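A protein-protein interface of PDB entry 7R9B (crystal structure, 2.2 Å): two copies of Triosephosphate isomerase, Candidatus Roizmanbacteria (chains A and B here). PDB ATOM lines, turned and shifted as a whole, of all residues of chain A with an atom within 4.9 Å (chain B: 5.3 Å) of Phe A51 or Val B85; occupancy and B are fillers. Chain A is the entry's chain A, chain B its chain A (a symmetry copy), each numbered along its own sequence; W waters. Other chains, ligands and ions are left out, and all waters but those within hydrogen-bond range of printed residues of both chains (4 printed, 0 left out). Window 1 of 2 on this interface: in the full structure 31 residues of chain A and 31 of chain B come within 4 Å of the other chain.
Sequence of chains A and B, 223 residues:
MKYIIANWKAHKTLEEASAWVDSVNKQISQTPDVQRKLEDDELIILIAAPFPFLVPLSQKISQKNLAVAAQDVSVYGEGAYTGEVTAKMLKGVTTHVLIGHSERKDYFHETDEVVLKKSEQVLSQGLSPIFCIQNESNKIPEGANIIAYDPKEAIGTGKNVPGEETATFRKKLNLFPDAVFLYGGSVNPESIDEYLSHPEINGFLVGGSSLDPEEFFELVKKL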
ATOM      1  N   ALA A  49      27.511 -14.150 -26.191  1.00  0.00           N
ATOM      2  CA  ALA A  49      28.391 -13.534 -25.201  1.00  0.00           C
ATOM      3  C   ALA A  49      28.382 -14.316 -23.889  1.00  0.00           C
ATOM      4  O   ALA A  49      27.366 -14.925 -23.534  1.00  0.00           O
ATOM      5  CB  ALA A  49      27.965 -12.091 -24.912  1.00  0.00           C
ATOM      6  N   PRO A  50      29.501 -14.295 -23.158  1.00  0.00           N
ATOM      7  CA  PRO A  50      29.537 -14.911 -21.822  1.00  0.00           C
ATOM      8  C   PRO A  50      28.411 -14.392 -20.941  1.00  0.00           C
ATOM      9  O   PRO A  50      28.038 -13.217 -21.014  1.00  0.00           O
ATOM     10  CB  PRO A  50      30.906 -14.497 -21.271  1.00  0.00           C
ATOM     11  CG  PRO A  50      31.773 -14.244 -22.526  1.00  0.00           C
ATOM     12  CD  PRO A  50      30.815 -13.758 -23.581  1.00  0.00           C
ATOM     13  N   PHE A  51      27.876 -15.300 -20.110  1.00  0.00           N
ATOM     14  CA  PHE A  51      26.784 -15.024 -19.165  1.00  0.00           C
ATOM     15  C   PHE A  51      26.833 -13.647 -18.507  1.00  0.00           C
ATOM     16  O   PHE A  51      25.811 -12.950 -18.542  1.00  0.00           O
ATOM     17  CB  PHE A  51      26.745 -16.099 -18.064  1.00  0.00           C
ATOM     18  CG  PHE A  51      26.346 -17.493 -18.534  1.00  0.00           C
ATOM     19  CD1 PHE A  51      25.224 -17.692 -19.318  1.00  0.00           C
ATOM     20  CD2 PHE A  51      27.078 -18.616 -18.124  1.00  0.00           C
ATOM     21  CE1 PHE A  51      24.855 -18.978 -19.725  1.00  0.00           C
ATOM     22  CE2 PHE A  51      26.719 -19.902 -18.530  1.00  0.00           C
ATOM     23  CZ  PHE A  51      25.597 -20.085 -19.333  1.00  0.00           C
ATOM     24  N   PRO A  52      27.938 -13.188 -17.896  1.00  0.00           N
ATOM     25  CA  PRO A  52      27.875 -11.892 -17.183  1.00  0.00           C
ATOM     26  C   PRO A  52      27.718 -10.676 -18.094  1.00  0.00           C
ATOM     27  O   PRO A  52      27.495  -9.566 -17.583  1.00  0.00           O
ATOM     28  CB  PRO A  52      29.201 -11.833 -16.412  1.00  0.00           C
ATOM     29  CG  PRO A  52      30.116 -12.748 -17.122  1.00  0.00           C
ATOM     30  CD  PRO A  52      29.261 -13.822 -17.767  1.00  0.00           C
ATOM     31  N   PHE A  53      27.814 -10.837 -19.415  1.00  0.00           N
ATOM     32  CA  PHE A  53      27.743  -9.704 -20.330  1.00  0.00           C
ATOM     33  C   PHE A  53      26.392  -9.574 -21.015  1.00  0.00           C
ATOM     34  O   PHE A  53      26.136  -8.546 -21.648  1.00  0.00           O
ATOM     35  CB  PHE A  53      28.836  -9.814 -21.400  1.00  0.00           C
ATOM     36  CG  PHE A  53      30.235  -9.882 -20.845  1.00  0.00           C
ATOM     37  CD1 PHE A  53      30.529  -9.373 -19.588  1.00  0.00           C
ATOM     38  CD2 PHE A  53      31.263 -10.456 -21.588  1.00  0.00           C
ATOM     39  CE1 PHE A  53      31.823  -9.437 -19.080  1.00  0.00           C
ATOM     40  CE2 PHE A  53      32.547 -10.520 -21.081  1.00  0.00           C
ATOM     41  CZ  PHE A  53      32.830 -10.009 -19.826  1.00  0.00           C
ATOM     42  N   LEU A  54      25.519 -10.575 -20.889  1.00  0.00           N
ATOM     43  CA  LEU A  54      24.300 -10.609 -21.689  1.00  0.00           C
ATOM     44  C   LEU A  54      23.436  -9.369 -21.459  1.00  0.00           C
ATOM     45  O   LEU A  54      22.974  -8.739 -22.416  1.00  0.00           O
ATOM     46  CB  LEU A  54      23.522 -11.892 -21.383  1.00  0.00           C
ATOM     47  CG  LEU A  54      24.224 -13.223 -21.705  1.00  0.00           C
ATOM     48  CD1 LEU A  54      23.381 -14.419 -21.283  1.00  0.00           C
ATOM     49  CD2 LEU A  54      24.532 -13.325 -23.186  1.00  0.00           C
ATOM     50  N   ALA A  70      22.929 -16.749 -25.304  1.00  0.00           N
ATOM     51  CA  ALA A  70      23.783 -17.461 -24.363  1.00  0.00           C
ATOM     52  C   ALA A  70      24.597 -18.512 -25.101  1.00  0.00           C
ATOM     53  O   ALA A  70      24.162 -19.054 -26.124  1.00  0.00           O
ATOM     54  CB  ALA A  70      22.945 -18.123 -23.264  1.00  0.00           C
ATOM     55  N   ASP A  72      25.551 -21.347 -23.551  1.00  0.00           N
ATOM     56  CA  ASP A  72      25.315 -22.612 -22.848  1.00  0.00           C
ATOM     57  C   ASP A  72      24.185 -22.377 -21.847  1.00  0.00           C
ATOM     58  O   ASP A  72      23.702 -21.254 -21.687  1.00  0.00           O
ATOM     59  CB  ASP A  72      26.599 -23.084 -22.157  1.00  0.00           C
ATOM     60  CG  ASP A  72      26.514 -24.508 -21.625  1.00  0.00           C
ATOM     61  OD1 ASP A  72      25.743 -25.341 -22.148  1.00  0.00           O
ATOM     62  OD2 ASP A  72      27.260 -24.798 -20.681  1.00  0.00           O
ATOM     63  N   VAL A  73      23.772 -23.439 -21.156  1.00  0.00           N
ATOM     64  CA  VAL A  73      22.753 -23.327 -20.120  1.00  0.00           C
ATOM     65  C   VAL A  73      22.848 -24.575 -19.247  1.00  0.00           C
ATOM     66  O   VAL A  73      23.412 -25.593 -19.654  1.00  0.00           O
ATOM     67  CB  VAL A  73      21.346 -23.152 -20.755  1.00  0.00           C
ATOM     68  CG1 VAL A  73      20.873 -24.450 -21.390  1.00  0.00           C
ATOM     69  CG2 VAL A  73      20.336 -22.660 -19.719  1.00  0.00           C
ATOM     70  N   VAL A  85      23.653 -21.563 -14.328  1.00  0.00           N
ATOM     71  CA  VAL A  85      22.762 -20.587 -14.953  1.00  0.00           C
ATOM     72  C   VAL A  85      21.681 -21.358 -15.699  1.00  0.00           C
ATOM     73  O   VAL A  85      21.981 -22.116 -16.635  1.00  0.00           O
ATOM     74  CB  VAL A  85      23.529 -19.629 -15.872  1.00  0.00           C
ATOM     75  CG1 VAL A  85      22.565 -18.616 -16.512  1.00  0.00           C
ATOM     76  CG2 VAL A  85      24.605 -18.920 -15.075  1.00  0.00           C
ATOM     77  N   LEU A  90      17.528 -17.235 -18.042  1.00  0.00           N
ATOM     78  CA  LEU A  90      17.767 -16.654 -19.357  1.00  0.00           C
ATOM     79  C   LEU A  90      16.474 -16.139 -19.984  1.00  0.00           C
ATOM     80  O   LEU A  90      16.521 -15.230 -20.825  1.00  0.00           O
ATOM     81  CB  LEU A  90      18.435 -17.686 -20.278  1.00  0.00           C
ATOM     82  CG  LEU A  90      19.819 -18.250 -19.883  1.00  0.00           C
ATOM     83  CD1 LEU A  90      20.352 -19.218 -20.925  1.00  0.00           C
ATOM     84  CD2 LEU A  90      20.859 -17.162 -19.635  1.00  0.00           C
ATOM     85  N   PHE B  51      25.789 -15.648 -12.590  1.00  0.00           N
ATOM     86  CA  PHE B  51      26.571 -14.885 -13.571  1.00  0.00           C
ATOM     87  C   PHE B  51      25.789 -13.805 -14.321  1.00  0.00           C
ATOM     88  O   PHE B  51      26.262 -12.663 -14.353  1.00  0.00           O
ATOM     89  CB  PHE B  51      27.212 -15.834 -14.600  1.00  0.00           C
ATOM     90  CG  PHE B  51      28.300 -16.746 -14.046  1.00  0.00           C
ATOM     91  CD1 PHE B  51      29.332 -16.248 -13.272  1.00  0.00           C
ATOM     92  CD2 PHE B  51      28.310 -18.111 -14.365  1.00  0.00           C
ATOM     93  CE1 PHE B  51      30.337 -17.091 -12.789  1.00  0.00           C
ATOM     94  CE2 PHE B  51      29.305 -18.961 -13.881  1.00  0.00           C
ATOM     95  CZ  PHE B  51      30.328 -18.447 -13.090  1.00  0.00           C
ATOM     96  N   PRO B  52      24.626 -14.068 -14.938  1.00  0.00           N
ATOM     97  CA  PRO B  52      23.984 -12.999 -15.738  1.00  0.00           C
ATOM     98  C   PRO B  52      23.431 -11.838 -14.912  1.00  0.00           C
ATOM     99  O   PRO B  52      23.021 -10.824 -15.501  1.00  0.00           O
ATOM    100  CB  PRO B  52      22.857 -13.728 -16.484  1.00  0.00           C
ATOM    101  CG  PRO B  52      22.577 -14.943 -15.697  1.00  0.00           C
ATOM    102  CD  PRO B  52      23.867 -15.330 -14.998  1.00  0.00           C
ATOM    103  N   VAL B  73      33.653 -20.126 -11.084  1.00  0.00           N
ATOM    104  CA  VAL B  73      34.467 -19.544 -12.146  1.00  0.00           C
ATOM    105  C   VAL B  73      35.087 -20.696 -12.931  1.00  0.00           C
ATOM    106  O   VAL B  73      35.163 -21.826 -12.445  1.00  0.00           O
ATOM    107  CB  VAL B  73      35.535 -18.587 -11.553  1.00  0.00           C
ATOM    108  CG1 VAL B  73      36.629 -19.368 -10.840  1.00  0.00           C
ATOM    109  CG2 VAL B  73      36.132 -17.692 -12.637  1.00  0.00           C
ATOM    110  N   SER B  74      35.502 -20.419 -14.168  1.00  0.00           N
ATOM    111  CA  SER B  74      36.060 -21.460 -15.034  1.00  0.00           C
ATOM    112  C   SER B  74      37.414 -21.957 -14.528  1.00  0.00           C
ATOM    113  O   SER B  74      38.212 -21.197 -13.965  1.00  0.00           O
ATOM    114  CB  SER B  74      36.218 -20.932 -16.464  1.00  0.00           C
ATOM    115  OG  SER B  74      36.587 -21.968 -17.363  1.00  0.00           O
ATOM    116  N   GLY B  83      31.002 -21.254 -23.435  1.00  0.00           N
ATOM    117  CA  GLY B  83      30.183 -21.398 -22.248  1.00  0.00           C
ATOM    118  C   GLY B  83      30.859 -21.016 -20.947  1.00  0.00           C
ATOM    119  O   GLY B  83      30.169 -20.837 -19.938  1.00  0.00           O
ATOM    120  N   GLU B  84      32.171 -20.859 -20.947  1.00  0.00           N
ATOM    121  CA  GLU B  84      32.925 -20.677 -19.718  1.00  0.00           C
ATOM    122  C   GLU B  84      32.959 -19.209 -19.322  1.00  0.00           C
ATOM    123  O   GLU B  84      33.103 -18.324 -20.171  1.00  0.00           O
ATOM    124  CB  GLU B  84      34.352 -21.202 -19.909  1.00  0.00           C
ATOM    125  CG  GLU B  84      34.459 -22.706 -19.846  1.00  0.00           C
ATOM    126  CD  GLU B  84      33.737 -23.267 -18.610  1.00  0.00           C
ATOM    127  OE1 GLU B  84      34.290 -23.155 -17.479  1.00  0.00           O
ATOM    128  OE2 GLU B  84      32.613 -23.802 -18.779  1.00  0.00           O
ATOM    129  N   VAL B  85      32.863 -18.951 -18.022  1.00  0.00           N
ATOM    130  CA  VAL B  85      33.063 -17.608 -17.482  1.00  0.00           C
ATOM    131  C   VAL B  85      34.374 -17.610 -16.708  1.00  0.00           C
ATOM    132  O   VAL B  85      34.519 -18.344 -15.718  1.00  0.00           O
ATOM    133  CB  VAL B  85      31.879 -17.166 -16.615  1.00  0.00           C
ATOM    134  CG1 VAL B  85      32.118 -15.752 -16.063  1.00  0.00           C
ATOM    135  CG2 VAL B  85      30.605 -17.217 -17.436  1.00  0.00           C
ATOM    136  N   THR B  86      35.342 -16.810 -17.180  1.00  0.00           N
ATOM    137  CA  THR B  86      36.702 -16.834 -16.665  1.00  0.00           C
ATOM    138  C   THR B  86      36.880 -15.799 -15.564  1.00  0.00           C
ATOM    139  O   THR B  86      36.132 -14.824 -15.467  1.00  0.00           O
ATOM    140  CB  THR B  86      37.732 -16.555 -17.771  1.00  0.00           C
ATOM    141  OG1 THR B  86      37.524 -15.238 -18.294  1.00  0.00           O
ATOM    142  CG2 THR B  86      37.660 -17.596 -18.909  1.00  0.00           C
ATOM    143  N   ALA B  87      37.921 -16.005 -14.753  1.00  0.00           N
ATOM    144  CA  ALA B  87      38.288 -15.014 -13.747  1.00  0.00           C
ATOM    145  C   ALA B  87      38.528 -13.645 -14.373  1.00  0.00           C
ATOM    146  O   ALA B  87      38.112 -12.618 -13.820  1.00  0.00           O
ATOM    147  CB  ALA B  87      39.530 -15.484 -12.987  1.00  0.00           C
ATOM    148  N   MET B  89      37.109 -12.311 -16.924  1.00  0.00           N
ATOM    149  CA  MET B  89      35.830 -11.647 -17.156  1.00  0.00           C
ATOM    150  C   MET B  89      35.249 -11.091 -15.860  1.00  0.00           C
ATOM    151  O   MET B  89      34.488 -10.113 -15.886  1.00  0.00           O
ATOM    152  CB  MET B  89      34.831 -12.638 -17.753  1.00  0.00           C
ATOM    153  CG  MET B  89      35.233 -13.245 -19.084  1.00  0.00           C
ATOM    154  SD  MET B  89      33.975 -14.453 -19.518  1.00  0.00           S
ATOM    155  CE  MET B  89      34.754 -15.225 -20.927  1.00  0.00           C
ATOM    156  N   LEU B  90      35.548 -11.741 -14.730  1.00  0.00           N
ATOM    157  CA  LEU B  90      35.005 -11.299 -13.450  1.00  0.00           C
ATOM    158  C   LEU B  90      35.792 -10.121 -12.886  1.00  0.00           C
ATOM    159  O   LEU B  90      35.239  -9.332 -12.106  1.00  0.00           O
ATOM    160  CB  LEU B  90      34.991 -12.465 -12.451  1.00  0.00           C
ATOM    161  CG  LEU B  90      34.149 -13.718 -12.780  1.00  0.00           C
ATOM    162  CD1 LEU B  90      34.212 -14.748 -11.664  1.00  0.00           C
ATOM    163  CD2 LEU B  90      32.689 -13.396 -13.079  1.00  0.00           C
HETATM  164  O   HOH W   1      26.410  -9.773 -15.198  1.00  0.00           O
HETATM  165  O   HOH W   2      28.319 -23.143 -18.823  1.00  0.00           O
HETATM  166  O   HOH W   3      24.089 -10.562 -17.888  1.00  0.00           O
HETATM  167  O   HOH W   4      28.804 -18.207 -20.756  1.00  0.00           O
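N of Ser B74 sits at hydrogen-bond distance from O of Val B85, 2.8 Å away.
The backbone NH of Met B89 sits close to the side-chain hydroxyl of Thr B86.
Among the printed residues, merely in contact across the chains: Pro A50 with Met B89 (3.5 Å), Phe A51 with Phe B51 (3.5 Å), Phe A51 with Pro B52 (3.3 Å), Phe A51 with Gly B83 (3.8 Å), Phe A51 with Val B85 (3.9 Å), Pro A52 with Phe B51 (3.3 Å), Pro A52 with Val B85 (3.7 Å), Phe A53 with Met B89 (3.9 Å), Asp A72 with Gly B83 (3.96 Å), Val A85 with Phe B51 (3.9 Å) and Val A85 with Pro B52 (3.7 Å).
Of chain B, only Phe B51 (3.5 Å), Pro B52 (3.3 Å), Gly B83 (3.8 Å) and Val B85 (3.9 Å) come within 4 Å of Phe A51.
Of chain A, only Phe A51 (3.9 Å) and Pro A52 (3.7 Å) come within 4 Å of Val B85.
Printed residues of chain B within 4 Å of Phe A53: Met B89 (3.9 Å).
Of the printed residues of chain B, Asp A72 touches Gly B83.
Of the printed residues of chain B, Val A85 touches Phe B51 (3.9 Å) and Pro B52 (3.7 Å).
Printed residues of chain A within 4 Å of Pro B52: Phe A51 and Val A85.
Printed residues of chain A within 4 Å of Gly B83: Phe A51 (3.8 Å) and Asp A72 (3.96 Å).
The nearest printed residue of chain B that does not touch Val A85 is Val B85 (6.7 Å).
Hydrophobic or aromatic side chains of chain A that line the printed part of chain B: Pro A50, Phe A51, Pro A52, Phe A53 and Val A85.
Of the 11 printed residues of chain B, 5 touch a printed residue of chain A.
Printed residues of chain B that touch a printed residue of chain A: Phe B51, Pro B52, Gly B83, Val B85 and Met B89.
Hydrophobic or aromatic side chains of chain B within 4 Å of the printed part of chain A: Phe B51, Pro B52, Val B85 and Met B89.
Among the printed residues, no Asp or Glu carboxylate lies within 4 Å of a Lys or Arg side-chain nitrogen of the other chain.
Phe A51 touches its own counterpart, Phe B51.
Phe A51 touches Pro B52, and with the chains exchanged Pro A52 touches Phe B51.
Phe A51 touches Val B85, and with the chains exchanged Val A85 touches Phe B51.
Pro A52 touches Val B85, and with the chains exchanged Val A85 touches Pro B52.
Positions printed for both chains: 51, 52, 73, 85 and 90.
Water W1 bridges the backbone carbonyl oxygen of Pro A52 (2.6 Å) and the backbone carbonyl oxygen of Phe B51 (3.0 Å).
Water W3 lies within hydrogen-bond range of the backbone carbonyl oxygen (O) of Pro B52, the backbone carbonyl oxygen (O) of Phe A51 and the backbone NH (N) of Leu A54.
Water W2 lies within hydrogen-bond range of the side-chain carboxylate (OD2) of Asp A72 (2.7 Å) and the backbone carbonyl oxygen (O) of Gly B83 (3.2 Å).
Water W4 bridges O of Gly B83 and N of Phe A51.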
